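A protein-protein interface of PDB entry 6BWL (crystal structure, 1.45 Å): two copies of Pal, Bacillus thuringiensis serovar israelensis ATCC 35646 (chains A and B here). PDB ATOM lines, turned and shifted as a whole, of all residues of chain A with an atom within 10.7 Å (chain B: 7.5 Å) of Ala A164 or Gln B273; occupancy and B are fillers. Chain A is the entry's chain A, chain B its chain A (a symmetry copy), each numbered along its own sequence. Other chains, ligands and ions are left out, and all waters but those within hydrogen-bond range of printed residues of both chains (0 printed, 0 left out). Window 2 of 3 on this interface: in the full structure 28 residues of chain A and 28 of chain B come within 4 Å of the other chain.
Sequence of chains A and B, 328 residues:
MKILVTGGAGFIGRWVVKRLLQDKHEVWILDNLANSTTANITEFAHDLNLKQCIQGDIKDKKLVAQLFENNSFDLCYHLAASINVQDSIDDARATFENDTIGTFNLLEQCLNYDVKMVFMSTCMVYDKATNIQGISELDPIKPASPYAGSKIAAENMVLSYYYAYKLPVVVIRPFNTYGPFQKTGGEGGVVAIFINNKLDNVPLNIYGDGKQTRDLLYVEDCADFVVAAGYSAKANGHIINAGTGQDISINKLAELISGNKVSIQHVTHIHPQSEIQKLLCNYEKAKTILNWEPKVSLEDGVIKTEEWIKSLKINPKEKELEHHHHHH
The backbone carbonyl oxygen of Ala A164 is in hydrogen-bond range of the side-chain amide nitrogen of Gln B273 (3.0 Å). OH of Tyr A165 lies within hydrogen-bond range of O of Ile B89, 2.6 Å away.
The backbone carbonyl oxygen (O) of Ala B144 lies within hydrogen-bond range of the side-chain hydroxyl (OG) of Ser B274 (2.7 Å). OG of Ser B88 lies within hydrogen-bond range of O of Val B85, at 2.7 Å. The side-chain hydroxyl (OG) of Ser A160 lies within hydrogen-bond range of the backbone carbonyl oxygen (O) of Met A157 (2.8 Å).
OD1 of Asn A156 touches CG of Pro B143, 3.4 Å away. CB of Ser A160 touches O of Ser B145, 3.4 Å away. Ser A160 touches Pro B146 (OG to CA, 3.6 Å). Tyr A163 touches Lys B142. Pro B143 touches Tyr A163. O of Tyr A163 touches CG of Gln B273 (3.3 Å). Ala A164 touches Ala B144. Ala A164 touches Pro B146 (CB to CD, 3.9 Å). Tyr A165 touches Ser B88. CG of Pro B146 touches OH of Tyr A165, at 3.8 Å.
Of the printed residues of chain B, Ala A164 touches Ala B144, Pro B146 and Gln B273. Of the printed residues of chain A, Ala B144 touches Tyr A163 and Ala A164. No residue of chain A comes within 4 Å of Pro B272. No residue of chain A comes within 4 Å of Ser B274. Printed residues of chain A within 4 Å of Pro B146: Ser A160, Ala A164 and Tyr A165. Of the printed residues of chain B, Ser A160 touches Pro B143, Ser B145 and Pro B146. Of the printed residues of chain A, Pro B143 touches Asn A156 (3.4 Å), Leu A159 (3.8 Å), Ser A160 (3.2 Å) and Tyr A163 (3.3 Å). Of the printed residues of chain A, Lys B142 touches Tyr A163 (3.4 Å). Pro A168 touches none of the printed residues of chain B. His B271 touches none of the printed residues of chain A. The nearest printed residue of chain A that does not touch Lys B142 is Asn A156 (5.5 Å).
Of the 18 printed residues of chain B, 8 touch a printed residue of chain A. Printed residues of chain B that touch a printed residue of chain A: Ser B88, Ile B89, Lys B142, Pro B143, Ala B144, Ser B145, Pro B146 and Gln B273. Hydrophobic or aromatic side chains of chain B that line the printed part of chain A: Ile B89, Pro B143 and Pro B146. Along chain B the printed residues that touch a printed residue of chain A span positions 88 to 273. Of the 18 printed residues of chain A, 6 touch a printed residue of chain B. Printed residues of chain A that touch a printed residue of chain B: Asn A156, Leu A159, Ser A160, Tyr A163, Ala A164 and Tyr A165. Hydrophobic or aromatic side chains of chain A that line the printed part of chain B: Leu A159, Tyr A163, Ala A164 and Tyr A165. Among the printed residues, no Asp or Glu carboxylate lies within 4 Å of a Lys or Arg side-chain nitrogen of the other chain.
No position is printed for both chains.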
ATOM      1  N   PHE A 104     -20.095  26.689 -36.759  1.00  0.00           N
ATOM      2  CA  PHE A 104     -19.669  25.318 -36.647  1.00  0.00           C
ATOM      3  C   PHE A 104     -18.400  25.040 -37.502  1.00  0.00           C
ATOM      4  O   PHE A 104     -17.450  24.382 -37.060  1.00  0.00           O
ATOM      5  CB  PHE A 104     -20.778  24.307 -37.016  1.00  0.00           C
ATOM      6  CG  PHE A 104     -20.323  22.885 -36.808  1.00  0.00           C
ATOM      7  CD1 PHE A 104     -20.315  22.350 -35.530  1.00  0.00           C
ATOM      8  CD2 PHE A 104     -19.764  22.165 -37.847  1.00  0.00           C
ATOM      9  CE1 PHE A 104     -19.816  21.085 -35.286  1.00  0.00           C
ATOM     10  CE2 PHE A 104     -19.274  20.908 -37.627  1.00  0.00           C
ATOM     11  CZ  PHE A 104     -19.284  20.380 -36.338  1.00  0.00           C
ATOM     12  N   LEU A 107     -15.518  26.398 -35.650  1.00  0.00           N
ATOM     13  CA  LEU A 107     -15.300  25.690 -34.408  1.00  0.00           C
ATOM     14  C   LEU A 107     -14.560  24.387 -34.650  1.00  0.00           C
ATOM     15  O   LEU A 107     -13.645  24.000 -33.898  1.00  0.00           O
ATOM     16  CB  LEU A 107     -16.696  25.476 -33.802  1.00  0.00           C
ATOM     17  CG  LEU A 107     -16.762  24.798 -32.471  1.00  0.00           C
ATOM     18  CD1 LEU A 107     -16.081  25.684 -31.401  1.00  0.00           C
ATOM     19  CD2 LEU A 107     -18.253  24.597 -32.159  1.00  0.00           C
ATOM     20  N   LEU A 111     -10.893  23.404 -32.959  1.00  0.00           N
ATOM     21  CA  LEU A 111     -10.533  22.176 -32.259  1.00  0.00           C
ATOM     22  C   LEU A 111      -9.304  21.545 -32.870  1.00  0.00           C
ATOM     23  O   LEU A 111      -8.386  21.177 -32.123  1.00  0.00           O
ATOM     24  CB  LEU A 111     -11.700  21.199 -32.262  1.00  0.00           C
ATOM     25  CG  LEU A 111     -11.429  19.876 -31.552  1.00  0.00           C
ATOM     26  CD1 LEU A 111     -11.201  20.104 -30.055  1.00  0.00           C
ATOM     27  CD2 LEU A 111     -12.574  18.910 -31.748  1.00  0.00           C
ATOM     28  N   ASN A 156     -24.473  27.003 -28.254  1.00  0.00           N
ATOM     29  CA  ASN A 156     -24.484  25.662 -27.686  1.00  0.00           C
ATOM     30  C   ASN A 156     -23.534  24.739 -28.368  1.00  0.00           C
ATOM     31  O   ASN A 156     -22.991  23.856 -27.693  1.00  0.00           O
ATOM     32  CB  ASN A 156     -25.910  25.135 -27.638  1.00  0.00           C
ATOM     33  CG  ASN A 156     -26.617  25.702 -26.460  1.00  0.00           C
ATOM     34  OD1 ASN A 156     -26.519  25.131 -25.376  1.00  0.00           O
ATOM     35  ND2 ASN A 156     -27.211  26.885 -26.612  1.00  0.00           N
ATOM     36  N   MET A 157     -23.289  24.905 -29.667  1.00  0.00           N
ATOM     37  CA  MET A 157     -22.210  24.158 -30.289  1.00  0.00           C
ATOM     38  C   MET A 157     -20.852  24.555 -29.724  1.00  0.00           C
ATOM     39  O   MET A 157     -20.022  23.697 -29.392  1.00  0.00           O
ATOM     40  CB  MET A 157     -22.252  24.290 -31.802  1.00  0.00           C
ATOM     41  CG  MET A 157     -23.518  23.739 -32.424  1.00  0.00           C
ATOM     42  SD  MET A 157     -24.035  22.099 -31.887  1.00  0.00           S
ATOM     43  CE  MET A 157     -22.607  21.127 -32.367  1.00  0.00           C
ATOM     44  N   VAL A 158     -20.625  25.859 -29.576  1.00  0.00           N
ATOM     45  CA  VAL A 158     -19.359  26.352 -29.032  1.00  0.00           C
ATOM     46  C   VAL A 158     -19.105  25.804 -27.625  1.00  0.00           C
ATOM     47  O   VAL A 158     -18.038  25.266 -27.342  1.00  0.00           O
ATOM     48  CB  VAL A 158     -19.376  27.894 -29.041  1.00  0.00           C
ATOM     49  CG1 VAL A 158     -18.172  28.462 -28.275  1.00  0.00           C
ATOM     50  CG2 VAL A 158     -19.390  28.412 -30.476  1.00  0.00           C
ATOM     51  N   LEU A 159     -20.104  25.914 -26.758  1.00  0.00           N
ATOM     52  CA  LEU A 159     -19.938  25.433 -25.387  1.00  0.00           C
ATOM     53  C   LEU A 159     -19.770  23.914 -25.358  1.00  0.00           C
ATOM     54  O   LEU A 159     -19.012  23.391 -24.527  1.00  0.00           O
ATOM     55  CB  LEU A 159     -21.069  25.876 -24.487  1.00  0.00           C
ATOM     56  CG  LEU A 159     -21.037  27.371 -24.182  1.00  0.00           C
ATOM     57  CD1 LEU A 159     -22.387  27.814 -23.657  1.00  0.00           C
ATOM     58  CD2 LEU A 159     -19.923  27.714 -23.207  1.00  0.00           C
ATOM     59  N   SER A 160     -20.417  23.197 -26.277  1.00  0.00           N
ATOM     60  CA  SER A 160     -20.231  21.747 -26.305  1.00  0.00           C
ATOM     61  C   SER A 160     -18.797  21.360 -26.525  1.00  0.00           C
ATOM     62  O   SER A 160     -18.366  20.292 -26.058  1.00  0.00           O
ATOM     63  CB  SER A 160     -21.151  21.035 -27.293  1.00  0.00           C
ATOM     64  OG  SER A 160     -20.709  21.111 -28.645  1.00  0.00           O
ATOM     65  N   TYR A 161     -18.040  22.166 -27.273  1.00  0.00           N
ATOM     66  CA  TYR A 161     -16.624  21.883 -27.493  1.00  0.00           C
ATOM     67  C   TYR A 161     -15.786  22.126 -26.247  1.00  0.00           C
ATOM     68  O   TYR A 161     -14.812  21.393 -25.993  1.00  0.00           O
ATOM     69  CB  TYR A 161     -16.082  22.664 -28.692  1.00  0.00           C
ATOM     70  CG  TYR A 161     -16.331  22.002 -30.037  1.00  0.00           C
ATOM     71  CD1 TYR A 161     -15.322  21.830 -30.955  1.00  0.00           C
ATOM     72  CD2 TYR A 161     -17.588  21.522 -30.407  1.00  0.00           C
ATOM     73  CE1 TYR A 161     -15.543  21.242 -32.191  1.00  0.00           C
ATOM     74  CE2 TYR A 161     -17.806  20.929 -31.624  1.00  0.00           C
ATOM     75  CZ  TYR A 161     -16.785  20.793 -32.528  1.00  0.00           C
ATOM     76  OH  TYR A 161     -17.008  20.203 -33.770  1.00  0.00           O
ATOM     77  N   TYR A 162     -16.146  23.130 -25.462  1.00  0.00           N
ATOM     78  CA  TYR A 162     -15.493  23.372 -24.172  1.00  0.00           C
ATOM     79  C   TYR A 162     -15.684  22.159 -23.253  1.00  0.00           C
ATOM     80  O   TYR A 162     -14.734  21.653 -22.666  1.00  0.00           O
ATOM     81  CB  TYR A 162     -16.047  24.635 -23.544  1.00  0.00           C
ATOM     82  CG  TYR A 162     -15.589  24.837 -22.128  1.00  0.00           C
ATOM     83  CD1 TYR A 162     -14.299  25.264 -21.849  1.00  0.00           C
ATOM     84  CD2 TYR A 162     -16.413  24.574 -21.061  1.00  0.00           C
ATOM     85  CE1 TYR A 162     -13.869  25.467 -20.543  1.00  0.00           C
ATOM     86  CE2 TYR A 162     -15.983  24.742 -19.756  1.00  0.00           C
ATOM     87  CZ  TYR A 162     -14.693  25.153 -19.518  1.00  0.00           C
ATOM     88  OH  TYR A 162     -14.271  25.401 -18.222  1.00  0.00           O
ATOM     89  N   TYR A 163     -16.912  21.652 -23.178  1.00  0.00           N
ATOM     90  CA  TYR A 163     -17.152  20.514 -22.305  1.00  0.00           C
ATOM     91  C   TYR A 163     -16.535  19.234 -22.832  1.00  0.00           C
ATOM     92  O   TYR A 163     -15.885  18.478 -22.055  1.00  0.00           O
ATOM     93  CB  TYR A 163     -18.660  20.336 -22.010  1.00  0.00           C
ATOM     94  CG  TYR A 163     -19.228  21.466 -21.189  1.00  0.00           C
ATOM     95  CD1 TYR A 163     -18.767  21.734 -19.902  1.00  0.00           C
ATOM     96  CD2 TYR A 163     -20.176  22.317 -21.707  1.00  0.00           C
ATOM     97  CE1 TYR A 163     -19.257  22.783 -19.154  1.00  0.00           C
ATOM     98  CE2 TYR A 163     -20.670  23.363 -20.984  1.00  0.00           C
ATOM     99  CZ  TYR A 163     -20.207  23.629 -19.714  1.00  0.00           C
ATOM    100  OH  TYR A 163     -20.740  24.676 -18.962  1.00  0.00           O
ATOM    101  N   ALA A 164     -16.751  18.918 -24.097  1.00  0.00           N
ATOM    102  CA  ALA A 164     -16.340  17.629 -24.621  1.00  0.00           C
ATOM    103  C   ALA A 164     -14.840  17.511 -24.785  1.00  0.00           C
ATOM    104  O   ALA A 164     -14.294  16.428 -24.597  1.00  0.00           O
ATOM    105  CB  ALA A 164     -17.034  17.340 -25.940  1.00  0.00           C
ATOM    106  N   TYR A 165     -14.180  18.628 -25.126  1.00  0.00           N
ATOM    107  CA  TYR A 165     -12.777  18.612 -25.533  1.00  0.00           C
ATOM    108  C   TYR A 165     -11.877  19.486 -24.689  1.00  0.00           C
ATOM    109  O   TYR A 165     -10.658  19.481 -24.927  1.00  0.00           O
ATOM    110  CB  TYR A 165     -12.621  19.056 -26.989  1.00  0.00           C
ATOM    111  CG  TYR A 165     -13.554  18.356 -27.959  1.00  0.00           C
ATOM    112  CD1 TYR A 165     -14.556  19.042 -28.637  1.00  0.00           C
ATOM    113  CD2 TYR A 165     -13.452  16.993 -28.183  1.00  0.00           C
ATOM    114  CE1 TYR A 165     -15.409  18.412 -29.499  1.00  0.00           C
ATOM    115  CE2 TYR A 165     -14.306  16.356 -29.059  1.00  0.00           C
ATOM    116  CZ  TYR A 165     -15.300  17.057 -29.703  1.00  0.00           C
ATOM    117  OH  TYR A 165     -16.184  16.429 -30.567  1.00  0.00           O
ATOM    118  N   LYS A 166     -12.415  20.262 -23.751  1.00  0.00           N
ATOM    119  CA  LYS A 166     -11.673  21.278 -23.003  1.00  0.00           C
ATOM    120  C   LYS A 166     -11.069  22.315 -23.923  1.00  0.00           C
ATOM    121  O   LYS A 166     -10.091  22.967 -23.587  1.00  0.00           O
ATOM    122  CB  LYS A 166     -10.597  20.643 -22.094  1.00  0.00           C
ATOM    123  CG  LYS A 166     -11.207  19.560 -21.207  1.00  0.00           C
ATOM    124  CD  LYS A 166     -10.144  18.915 -20.317  1.00  0.00           C
ATOM    125  CE  LYS A 166      -9.324  17.942 -21.158  1.00  0.00           C
ATOM    126  NZ  LYS A 166      -7.866  17.883 -20.842  1.00  0.00           N
ATOM    127  N   LEU A 167     -11.726  22.583 -25.045  1.00  0.00           N
ATOM    128  CA  LEU A 167     -11.286  23.680 -25.934  1.00  0.00           C
ATOM    129  C   LEU A 167     -11.640  25.002 -25.275  1.00  0.00           C
ATOM    130  O   LEU A 167     -12.792  25.241 -24.955  1.00  0.00           O
ATOM    131  CB  LEU A 167     -11.987  23.598 -27.293  1.00  0.00           C
ATOM    132  CG  LEU A 167     -11.591  24.685 -28.300  1.00  0.00           C
ATOM    133  CD1 LEU A 167     -10.146  24.505 -28.755  1.00  0.00           C
ATOM    134  CD2 LEU A 167     -12.549  24.665 -29.471  1.00  0.00           C
ATOM    135  N   PRO A 168     -10.680  25.922 -25.089  1.00  0.00           N
ATOM    136  CA  PRO A 168     -11.035  27.241 -24.589  1.00  0.00           C
ATOM    137  C   PRO A 168     -12.005  27.977 -25.507  1.00  0.00           C
ATOM    138  O   PRO A 168     -11.730  28.172 -26.694  1.00  0.00           O
ATOM    139  CB  PRO A 168      -9.673  27.969 -24.520  1.00  0.00           C
ATOM    140  CG  PRO A 168      -8.698  26.836 -24.273  1.00  0.00           C
ATOM    141  CD  PRO A 168      -9.224  25.755 -25.175  1.00  0.00           C
ATOM    142  N   VAL A 169     -13.119  28.387 -24.922  1.00  0.00           N
ATOM    143  CA  VAL A 169     -14.101  29.246 -25.619  1.00  0.00           C
ATOM    144  C   VAL A 169     -14.662  30.228 -24.625  1.00  0.00           C
ATOM    145  O   VAL A 169     -14.620  30.011 -23.409  1.00  0.00           O
ATOM    146  CB  VAL A 169     -15.287  28.435 -26.202  1.00  0.00           C
ATOM    147  CG1 VAL A 169     -14.786  27.283 -27.042  1.00  0.00           C
ATOM    148  CG2 VAL A 169     -16.246  27.972 -25.130  1.00  0.00           C
ATOM    149  N   GLY A 237     -14.950  29.014 -20.841  1.00  0.00           N
ATOM    150  CA  GLY A 237     -16.098  28.200 -20.452  1.00  0.00           C
ATOM    151  C   GLY A 237     -17.312  28.984 -20.033  1.00  0.00           C
ATOM    152  O   GLY A 237     -18.365  28.382 -19.790  1.00  0.00           O
ATOM    153  N   VAL B  85     -23.996   9.733 -27.693  1.00  0.00           N
ATOM    154  CA  VAL B  85     -23.120  10.750 -27.139  1.00  0.00           C
ATOM    155  C   VAL B  85     -21.672  10.533 -27.575  1.00  0.00           C
ATOM    156  O   VAL B  85     -20.996  11.467 -27.994  1.00  0.00           O
ATOM    157  CB  VAL B  85     -23.262  10.844 -25.615  1.00  0.00           C
ATOM    158  CG1 VAL B  85     -22.185  11.702 -24.951  1.00  0.00           C
ATOM    159  CG2 VAL B  85     -24.632  11.389 -25.227  1.00  0.00           C
ATOM    160  N   GLN B  86     -21.158   9.308 -27.415  1.00  0.00           N
ATOM    161  CA  GLN B  86     -19.756   9.113 -27.750  1.00  0.00           C
ATOM    162  C   GLN B  86     -19.461   9.390 -29.216  1.00  0.00           C
ATOM    163  O   GLN B  86     -18.428   9.992 -29.516  1.00  0.00           O
ATOM    164  CB  GLN B  86     -19.268   7.711 -27.364  1.00  0.00           C
ATOM    165  CG  GLN B  86     -17.762   7.525 -27.552  1.00  0.00           C
ATOM    166  CD  GLN B  86     -16.994   8.430 -26.641  1.00  0.00           C
ATOM    167  OE1 GLN B  86     -17.316   8.552 -25.477  1.00  0.00           O
ATOM    168  NE2 GLN B  86     -15.966   9.078 -27.144  1.00  0.00           N
ATOM    169  N   SER B  88     -20.884  11.523 -31.046  1.00  0.00           N
ATOM    170  CA  SER B  88     -20.885  12.973 -31.217  1.00  0.00           C
ATOM    171  C   SER B  88     -19.612  13.611 -30.730  1.00  0.00           C
ATOM    172  O   SER B  88     -19.213  14.657 -31.227  1.00  0.00           O
ATOM    173  CB  SER B  88     -22.089  13.597 -30.507  1.00  0.00           C
ATOM    174  OG  SER B  88     -21.890  13.801 -29.110  1.00  0.00           O
ATOM    175  N   ILE B  89     -18.957  13.011 -29.737  1.00  0.00           N
ATOM    176  CA  ILE B  89     -17.628  13.444 -29.326  1.00  0.00           C
ATOM    177  C   ILE B  89     -16.572  13.036 -30.329  1.00  0.00           C
ATOM    178  O   ILE B  89     -15.704  13.837 -30.661  1.00  0.00           O
ATOM    179  CB  ILE B  89     -17.299  12.870 -27.921  1.00  0.00           C
ATOM    180  CG1 ILE B  89     -18.289  13.351 -26.858  1.00  0.00           C
ATOM    181  CG2 ILE B  89     -15.863  13.197 -27.517  1.00  0.00           C
ATOM    182  CD1 ILE B  89     -18.223  12.633 -25.520  1.00  0.00           C
ATOM    183  N   ASP B  90     -16.667  11.814 -30.849  1.00  0.00           N
ATOM    184  CA  ASP B  90     -15.692  11.351 -31.836  1.00  0.00           C
ATOM    185  C   ASP B  90     -15.842  12.106 -33.158  1.00  0.00           C
ATOM    186  O   ASP B  90     -14.854  12.270 -33.886  1.00  0.00           O
ATOM    187  CB  ASP B  90     -15.903   9.851 -32.108  1.00  0.00           C
ATOM    188  CG  ASP B  90     -15.624   8.951 -30.894  1.00  0.00           C
ATOM    189  OD1 ASP B  90     -15.014   9.381 -29.903  1.00  0.00           O
ATOM    190  OD2 ASP B  90     -16.105   7.797 -30.960  1.00  0.00           O
ATOM    191  N   LYS B 142     -27.009  22.651 -20.202  1.00  0.00           N
ATOM    192  CA  LYS B 142     -25.577  22.493 -20.229  1.00  0.00           C
ATOM    193  C   LYS B 142     -25.238  21.537 -21.350  1.00  0.00           C
ATOM    194  O   LYS B 142     -25.455  20.318 -21.214  1.00  0.00           O
ATOM    195  CB  LYS B 142     -25.032  21.959 -18.903  1.00  0.00           C
ATOM    196  CG  LYS B 142     -23.529  21.819 -18.883  1.00  0.00           C
ATOM    197  CD  LYS B 142     -23.077  21.087 -17.617  1.00  0.00           C
ATOM    198  CE  LYS B 142     -21.617  20.734 -17.715  1.00  0.00           C
ATOM    199  NZ  LYS B 142     -21.256  19.730 -16.675  1.00  0.00           N
ATOM    200  N   PRO B 143     -24.707  22.025 -22.483  1.00  0.00           N
ATOM    201  CA  PRO B 143     -24.466  21.160 -23.639  1.00  0.00           C
ATOM    202  C   PRO B 143     -23.154  20.408 -23.463  1.00  0.00           C
ATOM    203  O   PRO B 143     -22.139  20.825 -23.963  1.00  0.00           O
ATOM    204  CB  PRO B 143     -24.446  22.148 -24.786  1.00  0.00           C
ATOM    205  CG  PRO B 143     -23.887  23.383 -24.199  1.00  0.00           C
ATOM    206  CD  PRO B 143     -24.534  23.448 -22.843  1.00  0.00           C
ATOM    207  N   ALA B 144     -23.157  19.296 -22.734  1.00  0.00           N
ATOM    208  CA  ALA B 144     -21.900  18.678 -22.302  1.00  0.00           C
ATOM    209  C   ALA B 144     -21.272  17.778 -23.376  1.00  0.00           C
ATOM    210  O   ALA B 144     -20.117  17.337 -23.235  1.00  0.00           O
ATOM    211  CB  ALA B 144     -22.097  17.918 -21.014  1.00  0.00           C
ATOM    212  N   SER B 145     -22.022  17.512 -24.447  1.00  0.00           N
ATOM    213  CA  SER B 145     -21.530  16.820 -25.623  1.00  0.00           C
ATOM    214  C   SER B 145     -22.054  17.516 -26.849  1.00  0.00           C
ATOM    215  O   SER B 145     -23.071  18.217 -26.782  1.00  0.00           O
ATOM    216  CB  SER B 145     -21.992  15.365 -25.656  1.00  0.00           C
ATOM    217  OG  SER B 145     -23.408  15.262 -25.767  1.00  0.00           O
ATOM    218  N   PRO B 146     -21.425  17.273 -28.004  1.00  0.00           N
ATOM    219  CA  PRO B 146     -22.002  17.847 -29.236  1.00  0.00           C
ATOM    220  C   PRO B 146     -23.397  17.321 -29.542  1.00  0.00           C
ATOM    221  O   PRO B 146     -24.176  18.044 -30.202  1.00  0.00           O
ATOM    222  CB  PRO B 146     -20.986  17.503 -30.308  1.00  0.00           C
ATOM    223  CG  PRO B 146     -19.730  17.466 -29.535  1.00  0.00           C
ATOM    224  CD  PRO B 146     -20.075  16.736 -28.281  1.00  0.00           C
ATOM    225  N   HIS B 269     -14.688   5.182 -17.489  1.00  0.00           N
ATOM    226  CA  HIS B 269     -15.773   5.911 -18.146  1.00  0.00           C
ATOM    227  C   HIS B 269     -15.313   6.388 -19.512  1.00  0.00           C
ATOM    228  O   HIS B 269     -14.215   6.951 -19.652  1.00  0.00           O
ATOM    229  CB  HIS B 269     -16.228   7.081 -17.289  1.00  0.00           C
ATOM    230  CG  HIS B 269     -17.620   7.523 -17.584  1.00  0.00           C
ATOM    231  ND1 HIS B 269     -18.004   8.019 -18.807  1.00  0.00           N
ATOM    232  CD2 HIS B 269     -18.703   7.565 -16.794  1.00  0.00           C
ATOM    233  CE1 HIS B 269     -19.286   8.326 -18.761  1.00  0.00           C
ATOM    234  NE2 HIS B 269     -19.737   8.073 -17.546  1.00  0.00           N
ATOM    235  N   ILE B 270     -16.138   6.172 -20.529  1.00  0.00           N
ATOM    236  CA  ILE B 270     -15.800   6.574 -21.893  1.00  0.00           C
ATOM    237  C   ILE B 270     -15.869   8.103 -22.125  1.00  0.00           C
ATOM    238  O   ILE B 270     -15.192   8.604 -23.016  1.00  0.00           O
ATOM    239  CB  ILE B 270     -16.643   5.839 -22.945  1.00  0.00           C
ATOM    240  CG1 ILE B 270     -18.114   5.827 -22.615  1.00  0.00           C
ATOM    241  CG2 ILE B 270     -16.109   4.425 -23.165  1.00  0.00           C
ATOM    242  CD1 ILE B 270     -19.006   5.442 -23.778  1.00  0.00           C
ATOM    243  N   HIS B 271     -16.636   8.816 -21.319  1.00  0.00           N
ATOM    244  CA  HIS B 271     -16.749  10.269 -21.463  1.00  0.00           C
ATOM    245  C   HIS B 271     -17.200  10.934 -20.183  1.00  0.00           C
ATOM    246  O   HIS B 271     -18.265  11.555 -20.115  1.00  0.00           O
ATOM    247  CB  HIS B 271     -17.642  10.670 -22.643  1.00  0.00           C
ATOM    248  CG  HIS B 271     -18.983  10.015 -22.703  1.00  0.00           C
ATOM    249  ND1 HIS B 271     -19.294   9.158 -23.727  1.00  0.00           N
ATOM    250  CD2 HIS B 271     -20.124  10.205 -22.004  1.00  0.00           C
ATOM    251  CE1 HIS B 271     -20.549   8.774 -23.613  1.00  0.00           C
ATOM    252  NE2 HIS B 271     -21.071   9.378 -22.570  1.00  0.00           N
ATOM    253  N   PRO B 272     -16.348  10.910 -19.169  1.00  0.00           N
ATOM    254  CA  PRO B 272     -16.772  11.453 -17.889  1.00  0.00           C
ATOM    255  C   PRO B 272     -17.030  12.971 -17.940  1.00  0.00           C
ATOM    256  O   PRO B 272     -17.811  13.517 -17.158  1.00  0.00           O
ATOM    257  CB  PRO B 272     -15.593  11.090 -16.955  1.00  0.00           C
ATOM    258  CG  PRO B 272     -14.440  10.916 -17.875  1.00  0.00           C
ATOM    259  CD  PRO B 272     -15.007  10.334 -19.149  1.00  0.00           C
ATOM    260  N   GLN B 273     -16.341  13.609 -18.885  1.00  0.00           N
ATOM    261  CA  GLN B 273     -16.489  15.040 -19.106  1.00  0.00           C
ATOM    262  C   GLN B 273     -17.858  15.412 -19.616  1.00  0.00           C
ATOM    263  O   GLN B 273     -18.268  16.582 -19.479  1.00  0.00           O
ATOM    264  CB  GLN B 273     -15.404  15.535 -20.052  1.00  0.00           C
ATOM    265  CG  GLN B 273     -15.582  15.276 -21.536  1.00  0.00           C
ATOM    266  CD  GLN B 273     -15.173  13.900 -22.024  1.00  0.00           C
ATOM    267  OE1 GLN B 273     -15.087  12.937 -21.229  1.00  0.00           O
ATOM    268  NE2 GLN B 273     -14.939  13.766 -23.304  1.00  0.00           N
ATOM    269  N   SER B 274     -18.589  14.453 -20.169  1.00  0.00           N
ATOM    270  CA  SER B 274     -19.897  14.702 -20.794  1.00  0.00           C
ATOM    271  C   SER B 274     -21.020  14.053 -20.024  1.00  0.00           C
ATOM    272  O   SER B 274     -22.194  14.132 -20.401  1.00  0.00           O
ATOM    273  CB  SER B 274     -19.909  14.229 -22.263  1.00  0.00           C
ATOM    274  OG  SER B 274     -18.954  14.892 -23.027  1.00  0.00           O
ATOM    275  N   GLU B 275     -20.687  13.382 -18.921  1.00  0.00           N
ATOM    276  CA  GLU B 275     -21.669  12.697 -18.108  1.00  0.00           C
ATOM    277  C   GLU B 275     -22.561  13.705 -17.385  1.00  0.00           C
ATOM    278  O   GLU B 275     -22.179  14.871 -17.187  1.00  0.00           O
ATOM    279  CB  GLU B 275     -20.942  11.753 -17.126  1.00  0.00           C
ATOM    280  CG  GLU B 275     -21.797  10.875 -16.229  1.00  0.00           C
ATOM    281  CD  GLU B 275     -22.728   9.970 -17.008  1.00  0.00           C
ATOM    282  OE1 GLU B 275     -23.757  10.488 -17.519  1.00  0.00           O
ATOM    283  OE2 GLU B 275     -22.452   8.754 -17.177  1.00  0.00           O
ATOM    284  N   ILE B 276     -23.763  13.268 -17.033  1.00  0.00           N
ATOM    285  CA  ILE B 276     -24.650  14.018 -16.171  1.00  0.00           C
ATOM    286  C   ILE B 276     -24.826  13.192 -14.913  1.00  0.00           C
ATOM    287  O   ILE B 276     -25.304  12.040 -14.937  1.00  0.00           O
ATOM    288  CB  ILE B 276     -25.998  14.354 -16.840  1.00  0.00           C
ATOM    289  CG1 ILE B 276     -25.792  15.014 -18.210  1.00  0.00           C
ATOM    290  CG2 ILE B 276     -26.860  15.156 -15.890  1.00  0.00           C
ATOM    291  CD1 ILE B 276     -27.083  15.221 -18.971  1.00  0.00           C
